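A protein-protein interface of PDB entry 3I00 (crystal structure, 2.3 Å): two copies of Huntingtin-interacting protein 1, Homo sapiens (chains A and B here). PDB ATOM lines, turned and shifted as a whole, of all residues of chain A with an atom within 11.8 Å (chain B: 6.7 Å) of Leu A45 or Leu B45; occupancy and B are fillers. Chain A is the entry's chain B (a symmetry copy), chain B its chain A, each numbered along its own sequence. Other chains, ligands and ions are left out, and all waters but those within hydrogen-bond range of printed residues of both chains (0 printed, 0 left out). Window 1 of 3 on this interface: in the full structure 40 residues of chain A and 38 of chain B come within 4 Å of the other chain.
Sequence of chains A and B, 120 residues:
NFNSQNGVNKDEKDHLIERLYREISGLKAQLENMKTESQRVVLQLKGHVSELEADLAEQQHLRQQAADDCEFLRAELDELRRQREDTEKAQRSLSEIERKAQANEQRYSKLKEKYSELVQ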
ATOM      1  N   THR A  36     -14.583 -21.708  22.166  1.00  0.00           N
ATOM      2  CA  THR A  36     -14.673 -20.857  23.340  1.00  0.00           C
ATOM      3  C   THR A  36     -14.378 -19.390  22.995  1.00  0.00           C
ATOM      4  O   THR A  36     -15.093 -18.497  23.444  1.00  0.00           O
ATOM      5  CB  THR A  36     -13.777 -21.364  24.487  1.00  0.00           C
ATOM      6  OG1 THR A  36     -14.266 -22.632  24.945  1.00  0.00           O
ATOM      7  CG2 THR A  36     -13.775 -20.388  25.662  1.00  0.00           C
ATOM      8  N   GLU A  37     -13.353 -19.141  22.184  1.00  0.00           N
ATOM      9  CA  GLU A  37     -12.994 -17.769  21.820  1.00  0.00           C
ATOM     10  C   GLU A  37     -14.079 -17.161  20.942  1.00  0.00           C
ATOM     11  O   GLU A  37     -14.449 -15.996  21.119  1.00  0.00           O
ATOM     12  CB  GLU A  37     -11.643 -17.721  21.111  1.00  0.00           C
ATOM     13  N   SER A  38     -14.593 -17.960  20.011  1.00  0.00           N
ATOM     14  CA  SER A  38     -15.610 -17.503  19.073  1.00  0.00           C
ATOM     15  C   SER A  38     -16.897 -17.141  19.812  1.00  0.00           C
ATOM     16  O   SER A  38     -17.477 -16.082  19.568  1.00  0.00           O
ATOM     17  CB  SER A  38     -15.872 -18.550  17.972  1.00  0.00           C
ATOM     18  OG  SER A  38     -17.188 -18.431  17.437  1.00  0.00           O
ATOM     19  N   GLN A  39     -17.338 -18.004  20.724  1.00  0.00           N
ATOM     20  CA  GLN A  39     -18.565 -17.721  21.474  1.00  0.00           C
ATOM     21  C   GLN A  39     -18.449 -16.409  22.253  1.00  0.00           C
ATOM     22  O   GLN A  39     -19.416 -15.671  22.403  1.00  0.00           O
ATOM     23  CB  GLN A  39     -18.928 -18.886  22.401  1.00  0.00           C
ATOM     24  CG  GLN A  39     -19.457 -20.124  21.663  1.00  0.00           C
ATOM     25  CD  GLN A  39     -19.635 -21.341  22.578  1.00  0.00           C
ATOM     26  OE1 GLN A  39     -19.797 -21.208  23.796  1.00  0.00           O
ATOM     27  NE2 GLN A  39     -19.611 -22.535  21.984  1.00  0.00           N
ATOM     28  N   ARG A  40     -17.240 -16.129  22.721  1.00  0.00           N
ATOM     29  CA  ARG A  40     -16.896 -14.928  23.479  1.00  0.00           C
ATOM     30  C   ARG A  40     -17.023 -13.649  22.642  1.00  0.00           C
ATOM     31  O   ARG A  40     -17.586 -12.661  23.112  1.00  0.00           O
ATOM     32  CB  ARG A  40     -15.464 -15.106  23.987  1.00  0.00           C
ATOM     33  CG  ARG A  40     -14.963 -14.189  25.075  1.00  0.00           C
ATOM     34  CD  ARG A  40     -13.514 -14.601  25.398  1.00  0.00           C
ATOM     35  NE  ARG A  40     -13.450 -15.595  26.471  1.00  0.00           N
ATOM     36  CZ  ARG A  40     -12.484 -16.503  26.622  1.00  0.00           C
ATOM     37  NH1 ARG A  40     -11.468 -16.590  25.750  1.00  0.00           N
ATOM     38  NH2 ARG A  40     -12.552 -17.346  27.653  1.00  0.00           N
ATOM     39  N   VAL A  41     -16.496 -13.664  21.416  1.00  0.00           N
ATOM     40  CA  VAL A  41     -16.586 -12.511  20.510  1.00  0.00           C
ATOM     41  C   VAL A  41     -18.015 -12.266  19.988  1.00  0.00           C
ATOM     42  O   VAL A  41     -18.498 -11.127  19.996  1.00  0.00           O
ATOM     43  CB  VAL A  41     -15.585 -12.610  19.306  1.00  0.00           C
ATOM     44  CG1 VAL A  41     -15.848 -13.857  18.470  1.00  0.00           C
ATOM     45  CG2 VAL A  41     -15.666 -11.359  18.421  1.00  0.00           C
ATOM     46  N   VAL A  42     -18.674 -13.339  19.553  1.00  0.00           N
ATOM     47  CA  VAL A  42     -20.016 -13.289  18.978  1.00  0.00           C
ATOM     48  C   VAL A  42     -21.038 -12.743  19.959  1.00  0.00           C
ATOM     49  O   VAL A  42     -21.873 -11.913  19.592  1.00  0.00           O
ATOM     50  CB  VAL A  42     -20.442 -14.674  18.463  1.00  0.00           C
ATOM     51  CG1 VAL A  42     -21.923 -14.701  18.139  1.00  0.00           C
ATOM     52  CG2 VAL A  42     -19.620 -15.040  17.217  1.00  0.00           C
ATOM     53  N   LEU A  43     -20.936 -13.205  21.207  1.00  0.00           N
ATOM     54  CA  LEU A  43     -21.756 -12.770  22.311  1.00  0.00           C
ATOM     55  C   LEU A  43     -21.634 -11.255  22.544  1.00  0.00           C
ATOM     56  O   LEU A  43     -22.636 -10.570  22.706  1.00  0.00           O
ATOM     57  CB  LEU A  43     -21.378 -13.591  23.564  1.00  0.00           C
ATOM     58  CG  LEU A  43     -22.210 -13.522  24.844  1.00  0.00           C
ATOM     59  CD1 LEU A  43     -22.509 -14.900  25.437  1.00  0.00           C
ATOM     60  CD2 LEU A  43     -21.527 -12.650  25.892  1.00  0.00           C
ATOM     61  N   GLN A  44     -20.407 -10.736  22.519  1.00  0.00           N
ATOM     62  CA  GLN A  44     -20.139  -9.305  22.715  1.00  0.00           C
ATOM     63  C   GLN A  44     -20.690  -8.460  21.553  1.00  0.00           C
ATOM     64  O   GLN A  44     -21.196  -7.353  21.777  1.00  0.00           O
ATOM     65  CB  GLN A  44     -18.628  -9.083  22.933  1.00  0.00           C
ATOM     66  CG  GLN A  44     -18.083  -7.661  22.718  1.00  0.00           C
ATOM     67  CD  GLN A  44     -17.867  -7.293  21.233  1.00  0.00           C
ATOM     68  OE1 GLN A  44     -18.485  -6.350  20.723  1.00  0.00           O
ATOM     69  NE2 GLN A  44     -16.993  -8.039  20.541  1.00  0.00           N
ATOM     70  N   LEU A  45     -20.591  -8.983  20.329  1.00  0.00           N
ATOM     71  CA  LEU A  45     -21.105  -8.302  19.132  1.00  0.00           C
ATOM     72  C   LEU A  45     -22.614  -8.228  19.113  1.00  0.00           C
ATOM     73  O   LEU A  45     -23.182  -7.198  18.746  1.00  0.00           O
ATOM     74  CB  LEU A  45     -20.635  -8.986  17.853  1.00  0.00           C
ATOM     75  CG  LEU A  45     -19.168  -8.715  17.489  1.00  0.00           C
ATOM     76  CD1 LEU A  45     -18.604  -9.851  16.646  1.00  0.00           C
ATOM     77  CD2 LEU A  45     -19.042  -7.374  16.796  1.00  0.00           C
ATOM     78  N   LYS A  46     -23.246  -9.333  19.503  1.00  0.00           N
ATOM     79  CA  LYS A  46     -24.695  -9.432  19.610  1.00  0.00           C
ATOM     80  C   LYS A  46     -25.253  -8.496  20.677  1.00  0.00           C
ATOM     81  O   LYS A  46     -26.313  -7.910  20.476  1.00  0.00           O
ATOM     82  CB  LYS A  46     -25.106 -10.874  19.897  1.00  0.00           C
ATOM     83  CG  LYS A  46     -25.219 -11.726  18.639  1.00  0.00           C
ATOM     84  CD  LYS A  46     -25.937 -13.021  18.949  1.00  0.00           C
ATOM     85  CE  LYS A  46     -26.436 -13.698  17.693  1.00  0.00           C
ATOM     86  NZ  LYS A  46     -25.622 -14.896  17.390  1.00  0.00           N
ATOM     87  N   GLY A  47     -24.542  -8.362  21.796  1.00  0.00           N
ATOM     88  CA  GLY A  47     -24.911  -7.416  22.853  1.00  0.00           C
ATOM     89  C   GLY A  47     -24.810  -5.969  22.382  1.00  0.00           C
ATOM     90  O   GLY A  47     -25.673  -5.155  22.696  1.00  0.00           O
ATOM     91  N   HIS A  48     -23.753  -5.656  21.635  1.00  0.00           N
ATOM     92  CA  HIS A  48     -23.575  -4.341  21.031  1.00  0.00           C
ATOM     93  C   HIS A  48     -24.690  -4.043  20.045  1.00  0.00           C
ATOM     94  O   HIS A  48     -25.183  -2.923  19.994  1.00  0.00           O
ATOM     95  CB  HIS A  48     -22.237  -4.251  20.280  1.00  0.00           C
ATOM     96  CG  HIS A  48     -21.736  -2.849  20.101  1.00  0.00           C
ATOM     97  ND1 HIS A  48     -20.448  -2.563  19.707  1.00  0.00           N
ATOM     98  CD2 HIS A  48     -22.340  -1.655  20.294  1.00  0.00           C
ATOM     99  CE1 HIS A  48     -20.285  -1.255  19.644  1.00  0.00           C
ATOM    100  NE2 HIS A  48     -21.419  -0.679  19.998  1.00  0.00           N
ATOM    101  N   VAL A  49     -25.061  -5.038  19.243  1.00  0.00           N
ATOM    102  CA  VAL A  49     -26.155  -4.884  18.285  1.00  0.00           C
ATOM    103  C   VAL A  49     -27.431  -4.436  19.020  1.00  0.00           C
ATOM    104  O   VAL A  49     -28.060  -3.440  18.650  1.00  0.00           O
ATOM    105  CB  VAL A  49     -26.376  -6.171  17.415  1.00  0.00           C
ATOM    106  CG1 VAL A  49     -27.792  -6.232  16.824  1.00  0.00           C
ATOM    107  CG2 VAL A  49     -25.350  -6.243  16.275  1.00  0.00           C
ATOM    108  N   SER A  50     -27.780  -5.142  20.086  1.00  0.00           N
ATOM    109  CA  SER A  50     -29.050  -4.878  20.726  1.00  0.00           C
ATOM    110  C   SER A  50     -29.059  -3.581  21.527  1.00  0.00           C
ATOM    111  O   SER A  50     -30.090  -2.938  21.602  1.00  0.00           O
ATOM    112  CB  SER A  50     -29.546  -6.081  21.512  1.00  0.00           C
ATOM    113  OG  SER A  50     -28.560  -6.563  22.368  1.00  0.00           O
ATOM    114  N   GLU A  51     -27.907  -3.171  22.061  1.00  0.00           N
ATOM    115  CA  GLU A  51     -27.758  -1.827  22.637  1.00  0.00           C
ATOM    116  C   GLU A  51     -27.878  -0.717  21.593  1.00  0.00           C
ATOM    117  O   GLU A  51     -28.433   0.334  21.860  1.00  0.00           O
ATOM    118  CB  GLU A  51     -26.417  -1.663  23.330  1.00  0.00           C
ATOM    119  CG  GLU A  51     -26.204  -0.254  23.862  1.00  0.00           C
ATOM    120  CD  GLU A  51     -24.811  -0.030  24.392  1.00  0.00           C
ATOM    121  OE1 GLU A  51     -24.604   1.004  25.084  1.00  0.00           O
ATOM    122  OE2 GLU A  51     -23.934  -0.894  24.120  1.00  0.00           O
ATOM    123  N   LEU A  52     -27.324  -0.953  20.414  1.00  0.00           N
ATOM    124  CA  LEU A  52     -27.466  -0.016  19.320  1.00  0.00           C
ATOM    125  C   LEU A  52     -28.921   0.076  18.885  1.00  0.00           C
ATOM    126  O   LEU A  52     -29.422   1.175  18.623  1.00  0.00           O
ATOM    127  CB  LEU A  52     -26.548  -0.388  18.149  1.00  0.00           C
ATOM    128  CG  LEU A  52     -25.070   0.040  18.253  1.00  0.00           C
ATOM    129  CD1 LEU A  52     -24.318  -0.424  17.032  1.00  0.00           C
ATOM    130  CD2 LEU A  52     -24.877   1.546  18.428  1.00  0.00           C
ATOM    131  N   GLU A  53     -29.590  -1.074  18.817  1.00  0.00           N
ATOM    132  CA  GLU A  53     -31.005  -1.140  18.465  1.00  0.00           C
ATOM    133  C   GLU A  53     -31.881  -0.442  19.514  1.00  0.00           C
ATOM    134  O   GLU A  53     -32.820   0.269  19.167  1.00  0.00           O
ATOM    135  CB  GLU A  53     -31.428  -2.600  18.238  1.00  0.00           C
ATOM    136  CG  GLU A  53     -30.900  -3.194  16.906  1.00  0.00           C
ATOM    137  CD  GLU A  53     -31.242  -4.668  16.695  1.00  0.00           C
ATOM    138  OE1 GLU A  53     -31.532  -5.378  17.689  1.00  0.00           O
ATOM    139  OE2 GLU A  53     -31.212  -5.123  15.526  1.00  0.00           O
ATOM    140  N   ALA A  54     -31.547  -0.632  20.787  1.00  0.00           N
ATOM    141  CA  ALA A  54     -32.187   0.086  21.894  1.00  0.00           C
ATOM    142  C   ALA A  54     -32.055   1.599  21.745  1.00  0.00           C
ATOM    143  O   ALA A  54     -33.026   2.319  21.940  1.00  0.00           O
ATOM    144  CB  ALA A  54     -31.616  -0.357  23.225  1.00  0.00           C
ATOM    145  N   ASP A  55     -30.858   2.072  21.406  1.00  0.00           N
ATOM    146  CA  ASP A  55     -30.599   3.511  21.223  1.00  0.00           C
ATOM    147  C   ASP A  55     -31.317   4.079  19.983  1.00  0.00           C
ATOM    148  O   ASP A  55     -31.677   5.248  19.970  1.00  0.00           O
ATOM    149  CB  ASP A  55     -29.101   3.791  21.090  1.00  0.00           C
ATOM    150  CG  ASP A  55     -28.318   3.512  22.364  1.00  0.00           C
ATOM    151  OD1 ASP A  55     -28.890   3.539  23.487  1.00  0.00           O
ATOM    152  OD2 ASP A  55     -27.095   3.284  22.226  1.00  0.00           O
ATOM    153  N   ARG B  40     -16.535 -15.501   9.408  1.00  0.00           N
ATOM    154  CA  ARG B  40     -17.642 -14.994   8.591  1.00  0.00           C
ATOM    155  C   ARG B  40     -18.732 -14.380   9.476  1.00  0.00           C
ATOM    156  O   ARG B  40     -19.169 -13.255   9.243  1.00  0.00           O
ATOM    157  CB  ARG B  40     -18.224 -16.109   7.710  1.00  0.00           C
ATOM    158  CG  ARG B  40     -19.070 -15.602   6.539  1.00  0.00           C
ATOM    159  CD  ARG B  40     -19.950 -16.704   5.926  1.00  0.00           C
ATOM    160  NE  ARG B  40     -20.946 -17.186   6.886  1.00  0.00           N
ATOM    161  CZ  ARG B  40     -22.114 -16.593   7.132  1.00  0.00           C
ATOM    162  NH1 ARG B  40     -22.469 -15.485   6.486  1.00  0.00           N
ATOM    163  NH2 ARG B  40     -22.935 -17.112   8.036  1.00  0.00           N
ATOM    164  N   VAL B  41     -19.166 -15.128  10.488  1.00  0.00           N
ATOM    165  CA  VAL B  41     -20.205 -14.683  11.407  1.00  0.00           C
ATOM    166  C   VAL B  41     -19.767 -13.390  12.123  1.00  0.00           C
ATOM    167  O   VAL B  41     -20.559 -12.463  12.295  1.00  0.00           O
ATOM    168  CB  VAL B  41     -20.565 -15.812  12.415  1.00  0.00           C
ATOM    169  CG1 VAL B  41     -21.383 -15.291  13.597  1.00  0.00           C
ATOM    170  CG2 VAL B  41     -21.307 -16.944  11.714  1.00  0.00           C
ATOM    171  N   VAL B  42     -18.497 -13.342  12.509  1.00  0.00           N
ATOM    172  CA  VAL B  42     -17.926 -12.219  13.241  1.00  0.00           C
ATOM    173  C   VAL B  42     -17.926 -10.972  12.374  1.00  0.00           C
ATOM    174  O   VAL B  42     -18.243  -9.883  12.850  1.00  0.00           O
ATOM    175  CB  VAL B  42     -16.492 -12.576  13.787  1.00  0.00           C
ATOM    176  CG1 VAL B  42     -15.693 -11.335  14.178  1.00  0.00           C
ATOM    177  CG2 VAL B  42     -16.607 -13.526  14.985  1.00  0.00           C
ATOM    178  N   LEU B  43     -17.600 -11.147  11.098  1.00  0.00           N
ATOM    179  CA  LEU B  43     -17.540 -10.049  10.150  1.00  0.00           C
ATOM    180  C   LEU B  43     -18.912  -9.476   9.775  1.00  0.00           C
ATOM    181  O   LEU B  43     -19.057  -8.261   9.577  1.00  0.00           O
ATOM    182  CB  LEU B  43     -16.804 -10.483   8.880  1.00  0.00           C
ATOM    183  CG  LEU B  43     -15.268 -10.497   8.866  1.00  0.00           C
ATOM    184  CD1 LEU B  43     -14.774 -11.215   7.617  1.00  0.00           C
ATOM    185  CD2 LEU B  43     -14.700  -9.100   8.929  1.00  0.00           C
ATOM    186  N   GLN B  44     -19.920 -10.332   9.658  1.00  0.00           N
ATOM    187  CA  GLN B  44     -21.245  -9.805   9.346  1.00  0.00           C
ATOM    188  C   GLN B  44     -21.841  -9.111  10.570  1.00  0.00           C
ATOM    189  O   GLN B  44     -22.559  -8.130  10.427  1.00  0.00           O
ATOM    190  CB  GLN B  44     -22.181 -10.846   8.677  1.00  0.00           C
ATOM    191  CG  GLN B  44     -23.051 -11.711   9.595  1.00  0.00           C
ATOM    192  CD  GLN B  44     -24.384 -11.051   9.990  1.00  0.00           C
ATOM    193  OE1 GLN B  44     -24.603 -10.710  11.162  1.00  0.00           O
ATOM    194  NE2 GLN B  44     -25.276 -10.881   9.013  1.00  0.00           N
ATOM    195  N   LEU B  45     -21.499  -9.594  11.770  1.00  0.00           N
ATOM    196  CA  LEU B  45     -21.951  -8.930  12.978  1.00  0.00           C
ATOM    197  C   LEU B  45     -21.305  -7.557  13.066  1.00  0.00           C
ATOM    198  O   LEU B  45     -21.981  -6.570  13.359  1.00  0.00           O
ATOM    199  CB  LEU B  45     -21.713  -9.762  14.242  1.00  0.00           C
ATOM    200  CG  LEU B  45     -22.805 -10.776  14.614  1.00  0.00           C
ATOM    201  CD1 LEU B  45     -22.245 -11.833  15.548  1.00  0.00           C
ATOM    202  CD2 LEU B  45     -24.036 -10.117  15.223  1.00  0.00           C
ATOM    203  N   LYS B  46     -20.011  -7.502  12.778  1.00  0.00           N
ATOM    204  CA  LYS B  46     -19.292  -6.231  12.728  1.00  0.00           C
ATOM    205  C   LYS B  46     -19.909  -5.249  11.725  1.00  0.00           C
ATOM    206  O   LYS B  46     -20.079  -4.081  12.050  1.00  0.00           O
ATOM    207  CB  LYS B  46     -17.800  -6.446  12.450  1.00  0.00           C
ATOM    208  CG  LYS B  46     -17.032  -6.995  13.639  1.00  0.00           C
ATOM    209  CD  LYS B  46     -15.565  -7.292  13.305  1.00  0.00           C
ATOM    210  CE  LYS B  46     -14.764  -7.486  14.580  1.00  0.00           C
ATOM    211  NZ  LYS B  46     -13.376  -7.888  14.298  1.00  0.00           N
ATOM    212  N   GLY B  47     -20.215  -5.724  10.514  1.00  0.00           N
ATOM    213  CA  GLY B  47     -20.931  -4.927   9.508  1.00  0.00           C
ATOM    214  C   GLY B  47     -22.275  -4.378   9.981  1.00  0.00           C
ATOM    215  O   GLY B  47     -22.600  -3.229   9.716  1.00  0.00           O
ATOM    216  N   HIS B  48     -23.040  -5.205  10.694  1.00  0.00           N
ATOM    217  CA  HIS B  48     -24.349  -4.841  11.227  1.00  0.00           C
ATOM    218  C   HIS B  48     -24.247  -3.731  12.266  1.00  0.00           C
ATOM    219  O   HIS B  48     -24.997  -2.767  12.183  1.00  0.00           O
ATOM    220  CB  HIS B  48     -25.059  -6.086  11.814  1.00  0.00           C
ATOM    221  CG  HIS B  48     -26.504  -5.877  12.176  1.00  0.00           C
ATOM    222  ND1 HIS B  48     -27.304  -4.917  11.587  1.00  0.00           N
ATOM    223  CD2 HIS B  48     -27.305  -6.547  13.039  1.00  0.00           C
ATOM    224  CE1 HIS B  48     -28.525  -4.995  12.085  1.00  0.00           C
ATOM    225  NE2 HIS B  48     -28.554  -5.980  12.963  1.00  0.00           N
ATOM    226  N   VAL B  49     -23.333  -3.857  13.238  1.00  0.00           N
ATOM    227  CA  VAL B  49     -23.188  -2.800  14.253  1.00  0.00           C
ATOM    228  C   VAL B  49     -22.700  -1.495  13.624  1.00  0.00           C
ATOM    229  O   VAL B  49     -23.112  -0.422  14.036  1.00  0.00           O
ATOM    230  CB  VAL B  49     -22.335  -3.170  15.553  1.00  0.00           C
ATOM    231  CG1 VAL B  49     -22.128  -4.676  15.735  1.00  0.00           C
ATOM    232  CG2 VAL B  49     -21.018  -2.404  15.626  1.00  0.00           C
ATOM    233  N   SER B  50     -21.833  -1.598  12.624  1.00  0.00           N
ATOM    234  CA  SER B  50     -21.371  -0.430  11.892  1.00  0.00           C
ATOM    235  C   SER B  50     -22.533   0.234  11.163  1.00  0.00           C
ATOM    236  O   SER B  50     -22.604   1.464  11.079  1.00  0.00           O
ATOM    237  CB  SER B  50     -20.262  -0.814  10.907  1.00  0.00           C
ATOM    238  OG  SER B  50     -19.726   0.336  10.293  1.00  0.00           O
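NE2 of Gln A44 lies within hydrogen-bond range of O of Val A41.
O of Lys A46 lies within hydrogen-bond range of OG of Ser A50 (3.2 Å).
Among the printed residues, pairs that only touch across the chains: Leu A52 with Val B49 (3.2 Å), Val A41 with Val B42 (3.6 Å), Val A49 with Val B49 (3.6 Å), Leu A45 with Lys B46 (3.8 Å), Glu A53 with His B48 (3.8 Å), Val A49 with His B48 (3.8 Å), Leu A45 with Val B42 (3.8 Å), Leu A45 with Leu B45 (3.8 Å), Val A42 with Leu B45 (3.9 Å) and Lys A46 with Leu B45 (3.96 Å).
Printed residues of chain B within 4 Å of Val A41: Val B42 (3.6 Å).
Of the printed residues of chain B, Val A42 touches Leu B45 (3.9 Å).
Printed residues of chain B within 4 Å of Lys A46: Leu B45 (3.96 Å).
Val B42 touches two residues of chain A.
Gln B44 touches none of the printed residues of chain A.
Printed residues of chain A within 4 Å of Leu B45: Val A42, Leu A45 and Lys A46.
Lys B46 touches one residue of chain A.
Of chain A, only Val A49 and Glu A53 come within 4 Å of His B48.
Of chain A, only Val A49 and Leu A52 come within 4 Å of Val B49.
The nearest residue of chain A that does not touch Leu B45 is Val A49 (4.2 Å).
Of the 20 printed residues of chain A, 7 touch a printed residue of chain B.
Printed residues of chain A that touch a printed residue of chain B: Val A41, Val A42, Leu A45, Lys A46, Val A49, Leu A52 and Glu A53.
Hydrophobic or aromatic side chains of chain A within 4 Å of the printed part of chain B: Val A41, Val A42, Leu A45, Val A49 and Leu A52.
Of the 11 printed residues of chain B, 5 touch a printed residue of chain A.
Val A41 touches Val B42, but with the chains exchanged Val A42 does not touch Val B41 (4.03 Å).
Val A42 touches Leu B45, and with the chains exchanged Leu A45 touches Val B42.
Val A49 touches His B48, but with the chains exchanged His A48 does not touch Val B49 (4.1 Å).
Val A49 touches its own counterpart, Val B49.
11 positions are printed for both chains.
Of the 10 pairs that touch across the chains among the printed residues, 6 have their exchanged pair printed and touching as well.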
